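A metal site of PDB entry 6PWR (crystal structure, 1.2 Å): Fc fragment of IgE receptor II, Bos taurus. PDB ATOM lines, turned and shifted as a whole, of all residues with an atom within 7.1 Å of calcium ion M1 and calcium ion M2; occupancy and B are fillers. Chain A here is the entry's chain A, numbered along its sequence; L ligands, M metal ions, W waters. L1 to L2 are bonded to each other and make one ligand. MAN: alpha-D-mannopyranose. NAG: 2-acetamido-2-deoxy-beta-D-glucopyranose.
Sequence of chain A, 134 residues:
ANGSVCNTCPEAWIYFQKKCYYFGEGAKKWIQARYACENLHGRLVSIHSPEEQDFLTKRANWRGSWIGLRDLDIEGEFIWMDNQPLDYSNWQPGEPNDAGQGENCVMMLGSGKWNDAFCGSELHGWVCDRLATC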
ATOM      1  N   ARG A  70      -0.554 -32.229  -0.492  1.00  0.00           N
ATOM      2  CA  ARG A  70      -1.676 -32.100   0.419  1.00  0.00           C
ATOM      3  C   ARG A  70      -1.194 -31.386   1.675  1.00  0.00           C
ATOM      4  O   ARG A  70      -0.024 -31.458   2.032  1.00  0.00           O
ATOM      5  CB  ARG A  70      -2.296 -33.457   0.767  1.00  0.00           C
ATOM      6  CG  ARG A  70      -1.510 -34.332   1.716  1.00  0.00           C
ATOM      7  CD  ARG A  70      -0.252 -34.886   1.063  1.00  0.00           C
ATOM      8  NE  ARG A  70       0.050 -36.210   1.580  1.00  0.00           N
ATOM      9  CZ  ARG A  70       1.246 -36.790   1.490  1.00  0.00           C
ATOM     10  NH1 ARG A  70       2.257 -36.135   0.928  1.00  0.00           N
ATOM     11  NH2 ARG A  70       1.422 -38.004   1.978  1.00  0.00           N
ATOM     12  N   ASP A  71      -2.117 -30.675   2.322  1.00  0.00           N
ATOM     13  CA  ASP A  71      -1.850 -30.088   3.636  1.00  0.00           C
ATOM     14  C   ASP A  71      -2.770 -30.707   4.680  1.00  0.00           C
ATOM     15  O   ASP A  71      -3.204 -30.043   5.619  1.00  0.00           O
ATOM     16  CB  ASP A  71      -1.879 -28.549   3.617  1.00  0.00           C
ATOM     17  CG  ASP A  71      -3.276 -27.953   3.441  1.00  0.00           C
ATOM     18  OD1 ASP A  71      -4.183 -28.609   2.890  1.00  0.00           O
ATOM     19  OD2 ASP A  71      -3.497 -26.791   3.863  1.00  0.00           O
ATOM     20  N   LEU A  72      -3.017 -32.002   4.533  1.00  0.00           N
ATOM     21  CA  LEU A  72      -3.911 -32.723   5.423  1.00  0.00           C
ATOM     22  C   LEU A  72      -3.418 -32.711   6.862  1.00  0.00           C
ATOM     23  O   LEU A  72      -4.221 -32.563   7.797  1.00  0.00           O
ATOM     24  CB  LEU A  72      -4.074 -34.159   4.936  1.00  0.00           C
ATOM     25  CG  LEU A  72      -5.106 -34.321   3.827  1.00  0.00           C
ATOM     26  CD1 LEU A  72      -4.965 -35.658   3.142  1.00  0.00           C
ATOM     27  CD2 LEU A  72      -6.497 -34.156   4.422  1.00  0.00           C
ATOM     28  N   ILE A  74      -1.027 -30.656   8.606  1.00  0.00           N
ATOM     29  CA  ILE A  74      -1.005 -29.323   9.190  1.00  0.00           C
ATOM     30  C   ILE A  74      -1.455 -28.362   8.108  1.00  0.00           C
ATOM     31  O   ILE A  74      -0.826 -28.297   7.037  1.00  0.00           O
ATOM     32  CB  ILE A  74       0.397 -28.946   9.700  1.00  0.00           C
ATOM     33  CG1 ILE A  74       0.872 -29.941  10.755  1.00  0.00           C
ATOM     34  CG2 ILE A  74       0.371 -27.533  10.270  1.00  0.00           C
ATOM     35  CD1 ILE A  74       0.129 -29.837  12.073  1.00  0.00           C
ATOM     36  N   GLU A  75      -2.518 -27.621   8.386  1.00  0.00           N
ATOM     37  CA  GLU A  75      -3.067 -26.688   7.413  1.00  0.00           C
ATOM     38  C   GLU A  75      -1.980 -25.706   6.967  1.00  0.00           C
ATOM     39  O   GLU A  75      -1.236 -25.158   7.791  1.00  0.00           O
ATOM     40  CB  GLU A  75      -4.227 -25.922   8.026  1.00  0.00           C
ATOM     41  CG  GLU A  75      -4.824 -24.864   7.113  1.00  0.00           C
ATOM     42  CD  GLU A  75      -5.394 -25.453   5.823  1.00  0.00           C
ATOM     43  OE1 GLU A  75      -5.797 -26.639   5.827  1.00  0.00           O
ATOM     44  OE2 GLU A  75      -5.428 -24.723   4.818  1.00  0.00           O
ATOM     45  N   GLY A  76      -1.898 -25.496   5.663  1.00  0.00           N
ATOM     46  CA  GLY A  76      -0.945 -24.591   5.085  1.00  0.00           C
ATOM     47  C   GLY A  76       0.455 -25.121   4.983  1.00  0.00           C
ATOM     48  O   GLY A  76       1.329 -24.435   4.441  1.00  0.00           O
ATOM     49  N   GLU A  77       0.716 -26.323   5.487  1.00  0.00           N
ATOM     50  CA  GLU A  77       2.022 -26.969   5.366  1.00  0.00           C
ATOM     51  C   GLU A  77       1.856 -28.088   4.353  1.00  0.00           C
ATOM     52  O   GLU A  77       1.422 -29.191   4.690  1.00  0.00           O
ATOM     53  CB  GLU A  77       2.492 -27.518   6.708  1.00  0.00           C
ATOM     54  CG  GLU A  77       2.768 -26.428   7.729  1.00  0.00           C
ATOM     55  CD  GLU A  77       3.506 -26.932   8.955  1.00  0.00           C
ATOM     56  OE1 GLU A  77       3.870 -28.132   8.994  1.00  0.00           O
ATOM     57  OE2 GLU A  77       3.716 -26.135   9.897  1.00  0.00           O
ATOM     58  N   PHE A  78       2.175 -27.803   3.099  1.00  0.00           N
ATOM     59  CA  PHE A  78       1.976 -28.803   2.070  1.00  0.00           C
ATOM     60  C   PHE A  78       3.133 -29.777   2.063  1.00  0.00           C
ATOM     61  O   PHE A  78       4.280 -29.415   2.322  1.00  0.00           O
ATOM     62  CB  PHE A  78       1.774 -28.146   0.701  1.00  0.00           C
ATOM     63  CG  PHE A  78       0.431 -27.518   0.569  1.00  0.00           C
ATOM     64  CD1 PHE A  78       0.219 -26.216   0.977  1.00  0.00           C
ATOM     65  CD2 PHE A  78      -0.641 -28.261   0.128  1.00  0.00           C
ATOM     66  CE1 PHE A  78      -1.030 -25.655   0.895  1.00  0.00           C
ATOM     67  CE2 PHE A  78      -1.892 -27.707   0.054  1.00  0.00           C
ATOM     68  CZ  PHE A  78      -2.083 -26.397   0.444  1.00  0.00           C
ATOM     69  N   GLY A  94      -4.354 -17.023  -6.638  1.00  0.00           N
ATOM     70  CA  GLY A  94      -5.287 -17.035  -5.546  1.00  0.00           C
ATOM     71  C   GLY A  94      -5.348 -18.345  -4.798  1.00  0.00           C
ATOM     72  O   GLY A  94      -5.925 -18.392  -3.713  1.00  0.00           O
ATOM     73  N   GLU A  95      -4.785 -19.399  -5.360  1.00  0.00           N
ATOM     74  CA  GLU A  95      -4.720 -20.690  -4.727  1.00  0.00           C
ATOM     75  C   GLU A  95      -3.365 -20.871  -4.057  1.00  0.00           C
ATOM     76  O   GLU A  95      -2.380 -20.229  -4.450  1.00  0.00           O
ATOM     77  CB  GLU A  95      -4.891 -21.808  -5.768  1.00  0.00           C
ATOM     78  CG  GLU A  95      -6.137 -21.678  -6.612  1.00  0.00           C
ATOM     79  CD  GLU A  95      -7.434 -21.732  -5.832  1.00  0.00           C
ATOM     80  OE1 GLU A  95      -7.450 -22.220  -4.680  1.00  0.00           O
ATOM     81  OE2 GLU A  95      -8.451 -21.273  -6.400  1.00  0.00           O
ATOM     82  N   PRO A  96      -3.261 -21.712  -3.036  1.00  0.00           N
ATOM     83  CA  PRO A  96      -4.383 -22.405  -2.407  1.00  0.00           C
ATOM     84  C   PRO A  96      -5.182 -21.431  -1.556  1.00  0.00           C
ATOM     85  O   PRO A  96      -4.608 -20.506  -0.958  1.00  0.00           O
ATOM     86  CB  PRO A  96      -3.685 -23.443  -1.524  1.00  0.00           C
ATOM     87  CG  PRO A  96      -2.377 -22.802  -1.182  1.00  0.00           C
ATOM     88  CD  PRO A  96      -1.974 -22.003  -2.375  1.00  0.00           C
ATOM     89  N   ASN A  97      -6.487 -21.608  -1.545  1.00  0.00           N
ATOM     90  CA  ASN A  97      -7.363 -20.710  -0.815  1.00  0.00           C
ATOM     91  C   ASN A  97      -8.151 -21.365   0.304  1.00  0.00           C
ATOM     92  O   ASN A  97      -8.909 -20.674   0.993  1.00  0.00           O
ATOM     93  CB  ASN A  97      -8.300 -19.943  -1.759  1.00  0.00           C
ATOM     94  CG  ASN A  97      -9.265 -20.844  -2.495  1.00  0.00           C
ATOM     95  OD1 ASN A  97      -9.255 -22.063  -2.330  1.00  0.00           O
ATOM     96  ND2 ASN A  97     -10.122 -20.245  -3.305  1.00  0.00           N
ATOM     97  N   ASP A  98      -7.967 -22.668   0.520  1.00  0.00           N
ATOM     98  CA  ASP A  98      -8.639 -23.415   1.584  1.00  0.00           C
ATOM     99  C   ASP A  98     -10.138 -23.089   1.647  1.00  0.00           C
ATOM    100  O   ASP A  98     -10.684 -22.768   2.706  1.00  0.00           O
ATOM    101  CB  ASP A  98      -7.966 -23.208   2.939  1.00  0.00           C
ATOM    102  CG  ASP A  98      -8.230 -24.360   3.890  1.00  0.00           C
ATOM    103  OD1 ASP A  98      -8.073 -25.520   3.472  1.00  0.00           O
ATOM    104  OD2 ASP A  98      -8.603 -24.099   5.052  1.00  0.00           O
ATOM    105  N   ALA A  99     -10.783 -23.160   0.490  1.00  0.00           N
ATOM    106  CA  ALA A  99     -12.146 -22.684   0.344  1.00  0.00           C
ATOM    107  C   ALA A  99     -13.139 -23.611   1.036  1.00  0.00           C
ATOM    108  O   ALA A  99     -12.830 -24.741   1.420  1.00  0.00           O
ATOM    109  CB  ALA A  99     -12.508 -22.543  -1.130  1.00  0.00           C
ATOM    110  N   GLY A 102     -12.788 -26.363   3.835  1.00  0.00           N
ATOM    111  CA  GLY A 102     -11.394 -26.730   3.925  1.00  0.00           C
ATOM    112  C   GLY A 102     -11.015 -27.563   2.719  1.00  0.00           C
ATOM    113  O   GLY A 102     -11.715 -28.506   2.350  1.00  0.00           O
ATOM    114  N   GLU A 103      -9.914 -27.196   2.087  1.00  0.00           N
ATOM    115  CA  GLU A 103      -9.425 -27.868   0.893  1.00  0.00           C
ATOM    116  C   GLU A 103      -7.996 -28.278   1.190  1.00  0.00           C
ATOM    117  O   GLU A 103      -7.121 -27.421   1.349  1.00  0.00           O
ATOM    118  CB  GLU A 103      -9.507 -26.938  -0.307  1.00  0.00           C
ATOM    119  CG  GLU A 103     -10.938 -26.566  -0.642  1.00  0.00           C
ATOM    120  CD  GLU A 103     -11.045 -25.733  -1.887  1.00  0.00           C
ATOM    121  OE1 GLU A 103     -10.239 -24.805  -2.042  1.00  0.00           O
ATOM    122  OE2 GLU A 103     -11.928 -26.013  -2.727  1.00  0.00           O
ATOM    123  N   ASN A 104      -7.770 -29.575   1.276  1.00  0.00           N
ATOM    124  CA  ASN A 104      -6.493 -30.054   1.761  1.00  0.00           C
ATOM    125  C   ASN A 104      -5.750 -30.946   0.796  1.00  0.00           C
ATOM    126  O   ASN A 104      -4.676 -31.451   1.142  1.00  0.00           O
ATOM    127  CB  ASN A 104      -6.671 -30.728   3.124  1.00  0.00           C
ATOM    128  CG  ASN A 104      -7.377 -29.835   4.111  1.00  0.00           C
ATOM    129  OD1 ASN A 104      -7.153 -28.623   4.141  1.00  0.00           O
ATOM    130  ND2 ASN A 104      -8.258 -30.417   4.899  1.00  0.00           N
ATOM    131  N   CYS A 105      -6.288 -31.144  -0.395  1.00  0.00           N
ATOM    132  CA  CYS A 105      -5.684 -32.012  -1.392  1.00  0.00           C
ATOM    133  C   CYS A 105      -5.534 -31.227  -2.678  1.00  0.00           C
ATOM    134  O   CYS A 105      -6.449 -30.489  -3.074  1.00  0.00           O
ATOM    135  CB  CYS A 105      -6.578 -33.234  -1.635  1.00  0.00           C
ATOM    136  SG  CYS A 105      -6.618 -34.335  -0.216  1.00  0.00           S
ATOM    137  N   TRP A 114      -2.260 -25.352 -10.286  1.00  0.00           N
ATOM    138  CA  TRP A 114      -2.649 -26.126  -9.123  1.00  0.00           C
ATOM    139  C   TRP A 114      -3.757 -25.418  -8.357  1.00  0.00           C
ATOM    140  O   TRP A 114      -3.776 -24.194  -8.247  1.00  0.00           O
ATOM    141  CB  TRP A 114      -1.476 -26.325  -8.177  1.00  0.00           C
ATOM    142  CG  TRP A 114      -0.263 -26.945  -8.762  1.00  0.00           C
ATOM    143  CD1 TRP A 114      -0.115 -27.527  -9.976  1.00  0.00           C
ATOM    144  CD2 TRP A 114       1.001 -27.014  -8.112  1.00  0.00           C
ATOM    145  NE1 TRP A 114       1.184 -27.980 -10.134  1.00  0.00           N
ATOM    146  CE2 TRP A 114       1.890 -27.659  -9.001  1.00  0.00           C
ATOM    147  CE3 TRP A 114       1.475 -26.585  -6.874  1.00  0.00           C
ATOM    148  CZ2 TRP A 114       3.221 -27.886  -8.682  1.00  0.00           C
ATOM    149  CZ3 TRP A 114       2.792 -26.822  -6.553  1.00  0.00           C
ATOM    150  CH2 TRP A 114       3.652 -27.455  -7.450  1.00  0.00           C
ATOM    151  N   ASN A 115      -4.664 -26.220  -7.809  1.00  0.00           N
ATOM    152  CA  ASN A 115      -5.730 -25.718  -6.970  1.00  0.00           C
ATOM    153  C   ASN A 115      -5.858 -26.671  -5.791  1.00  0.00           C
ATOM    154  O   ASN A 115      -5.833 -27.891  -5.982  1.00  0.00           O
ATOM    155  CB  ASN A 115      -7.032 -25.733  -7.755  1.00  0.00           C
ATOM    156  CG  ASN A 115      -8.224 -25.425  -6.891  1.00  0.00           C
ATOM    157  OD1 ASN A 115      -8.195 -24.474  -6.117  1.00  0.00           O
ATOM    158  ND2 ASN A 115      -9.281 -26.240  -7.001  1.00  0.00           N
ATOM    159  N   ASP A 116      -6.007 -26.141  -4.588  1.00  0.00           N
ATOM    160  CA  ASP A 116      -6.431 -26.994  -3.495  1.00  0.00           C
ATOM    161  C   ASP A 116      -7.923 -27.257  -3.593  1.00  0.00           C
ATOM    162  O   ASP A 116      -8.716 -26.368  -3.900  1.00  0.00           O
ATOM    163  CB  ASP A 116      -6.051 -26.436  -2.116  1.00  0.00           C
ATOM    164  CG  ASP A 116      -6.627 -25.051  -1.826  1.00  0.00           C
ATOM    165  OD1 ASP A 116      -7.020 -24.324  -2.760  1.00  0.00           O
ATOM    166  OD2 ASP A 116      -6.631 -24.708  -0.623  1.00  0.00           O
ATOM    167  N   ALA A 117      -8.301 -28.505  -3.347  1.00  0.00           N
ATOM    168  CA  ALA A 117      -9.689 -28.908  -3.465  1.00  0.00           C
ATOM    169  C   ALA A 117     -10.064 -29.749  -2.265  1.00  0.00           C
ATOM    170  O   ALA A 117      -9.213 -30.285  -1.550  1.00  0.00           O
ATOM    171  CB  ALA A 117      -9.934 -29.701  -4.753  1.00  0.00           C
ATOM    172  N   PHE A 118     -11.370 -29.885  -2.072  1.00  0.00           N
ATOM    173  CA  PHE A 118     -11.886 -30.808  -1.082  1.00  0.00           C
ATOM    174  C   PHE A 118     -11.392 -32.214  -1.410  1.00  0.00           C
ATOM    175  O   PHE A 118     -11.548 -32.699  -2.529  1.00  0.00           O
ATOM    176  CB  PHE A 118     -13.405 -30.764  -1.106  1.00  0.00           C
ATOM    177  CG  PHE A 118     -14.066 -31.828  -0.287  1.00  0.00           C
ATOM    178  CD1 PHE A 118     -13.660 -32.095   0.998  1.00  0.00           C
ATOM    179  CD2 PHE A 118     -15.112 -32.567  -0.818  1.00  0.00           C
ATOM    180  CE1 PHE A 118     -14.291 -33.080   1.759  1.00  0.00           C
ATOM    181  CE2 PHE A 118     -15.734 -33.548  -0.080  1.00  0.00           C
ATOM    182  CZ  PHE A 118     -15.314 -33.805   1.204  1.00  0.00           C
HETATM  183  C1  MAN L   1     -13.979 -23.686  -6.987  1.00  0.00           C
HETATM  184  C2  MAN L   1     -13.024 -24.736  -6.380  1.00  0.00           C
HETATM  185  C3  MAN L   1     -12.058 -24.055  -5.421  1.00  0.00           C
HETATM  186  C4  MAN L   1     -11.339 -22.936  -6.118  1.00  0.00           C
HETATM  187  C5  MAN L   1     -12.360 -21.913  -6.620  1.00  0.00           C
HETATM  188  C6  MAN L   1     -11.713 -20.774  -7.382  1.00  0.00           C
HETATM  189  O1  MAN L   1     -14.834 -23.304  -5.955  1.00  0.00           O
HETATM  190  O2  MAN L   1     -12.191 -25.238  -7.394  1.00  0.00           O
HETATM  191  O3  MAN L   1     -11.085 -24.952  -4.917  1.00  0.00           O
HETATM  192  O4  MAN L   1     -10.436 -22.329  -5.217  1.00  0.00           O
HETATM  193  O5  MAN L   1     -13.270 -22.586  -7.531  1.00  0.00           O
HETATM  194  O6  MAN L   1     -12.733 -19.842  -7.761  1.00  0.00           O
HETATM  195  C1  NAG L   2     -12.793 -26.312  -8.104  1.00  0.00           C
HETATM  196  C2  NAG L   2     -12.151 -26.362  -9.487  1.00  0.00           C
HETATM  197  C3  NAG L   2     -12.719 -27.533 -10.274  1.00  0.00           C
HETATM  198  C4  NAG L   2     -12.608 -28.827  -9.463  1.00  0.00           C
HETATM  199  C5  NAG L   2     -13.160 -28.646  -8.058  1.00  0.00           C
HETATM  200  C6  NAG L   2     -12.896 -29.839  -7.174  1.00  0.00           C
HETATM  201  C7  NAG L   2     -11.459 -24.100 -10.171  1.00  0.00           C
HETATM  202  C8  NAG L   2     -11.826 -22.881 -10.964  1.00  0.00           C
HETATM  203  N2  NAG L   2     -12.346 -25.111 -10.200  1.00  0.00           N
HETATM  204  O3  NAG L   2     -11.988 -27.670 -11.484  1.00  0.00           O
HETATM  205  O4  NAG L   2     -13.341 -29.849 -10.117  1.00  0.00           O
HETATM  206  O5  NAG L   2     -12.541 -27.518  -7.420  1.00  0.00           O
HETATM  207  O6  NAG L   2     -13.579 -29.737  -5.931  1.00  0.00           O
HETATM  208  O7  NAG L   2     -10.404 -24.185  -9.550  1.00  0.00           O
HETATM  209 CA    CA M   1      -5.910 -26.709   3.345  1.00  0.00          CA
HETATM  210 CA    CA M   2      -9.042 -23.928  -3.903  1.00  0.00          CA
HETATM  211  O   HOH W   1      -5.231 -25.208   1.652  1.00  0.00           O
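The backbone NH of Asp 98 is in hydrogen-bond range of the side-chain carboxylate of Asp 116, 2.7 Å away.
The side-chain carboxylate (OE1) of Glu 103 sits close to the backbone NH (N) of Ala 99 (3.1 Å).
The backbone NH (N) of Asn 104 lies within hydrogen-bond range of the backbone carbonyl oxygen (O) of Ala 117 (3.3 Å).
The side-chain amide oxygen (OD1) of Asn 97 sits close to the backbone NH (N) of Ala 99 (3.4 Å).
OD2 of Asp 71 lies close to N of Gly 76, at 2.7 Å.
Along chain A the residues within 4 Å of calcium ion M1 span positions 71 to 104.
The nearest printed residue that does not touch calcium ion M1 is Asp 116 (4.5 Å).
Of the 23 residues printed, 5 come within 4 Å of calcium ion M2.
The nearest printed residue that does not touch calcium ion M2 is Ala 99 (4.6 Å).
Calcium ion M1 is bound by water W1, OD1 of Asn 104, O of Glu 103, OD2 of Asp 71, OD1 of Asp 98, OE1 of Glu 75, OE2 of Glu 75 and OD1 of Asp 71.
Calcium ion M1 has eight donor atoms within binding distance.
OD1 of Asp 116 is bound to calcium ion M2, at 2.4 Å.
Calcium ion M2 is bound by the side-chain carboxylate (OE1) of Glu 103 (2.4 Å).
Calcium ion M2 is bound by OD1 of Asn 115 (2.4 Å).
OD1 of Asn 97 binds calcium ion M2 (2.4 Å).
Calcium ion M2 is bound by OE1 of Glu 95 (2.5 Å).
Calcium ion M2 is bound by O of Asp 116 (2.5 Å).
O4 of MAN L1 binds calcium ion M2.
O3 of MAN L1 is bound to calcium ion M2.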
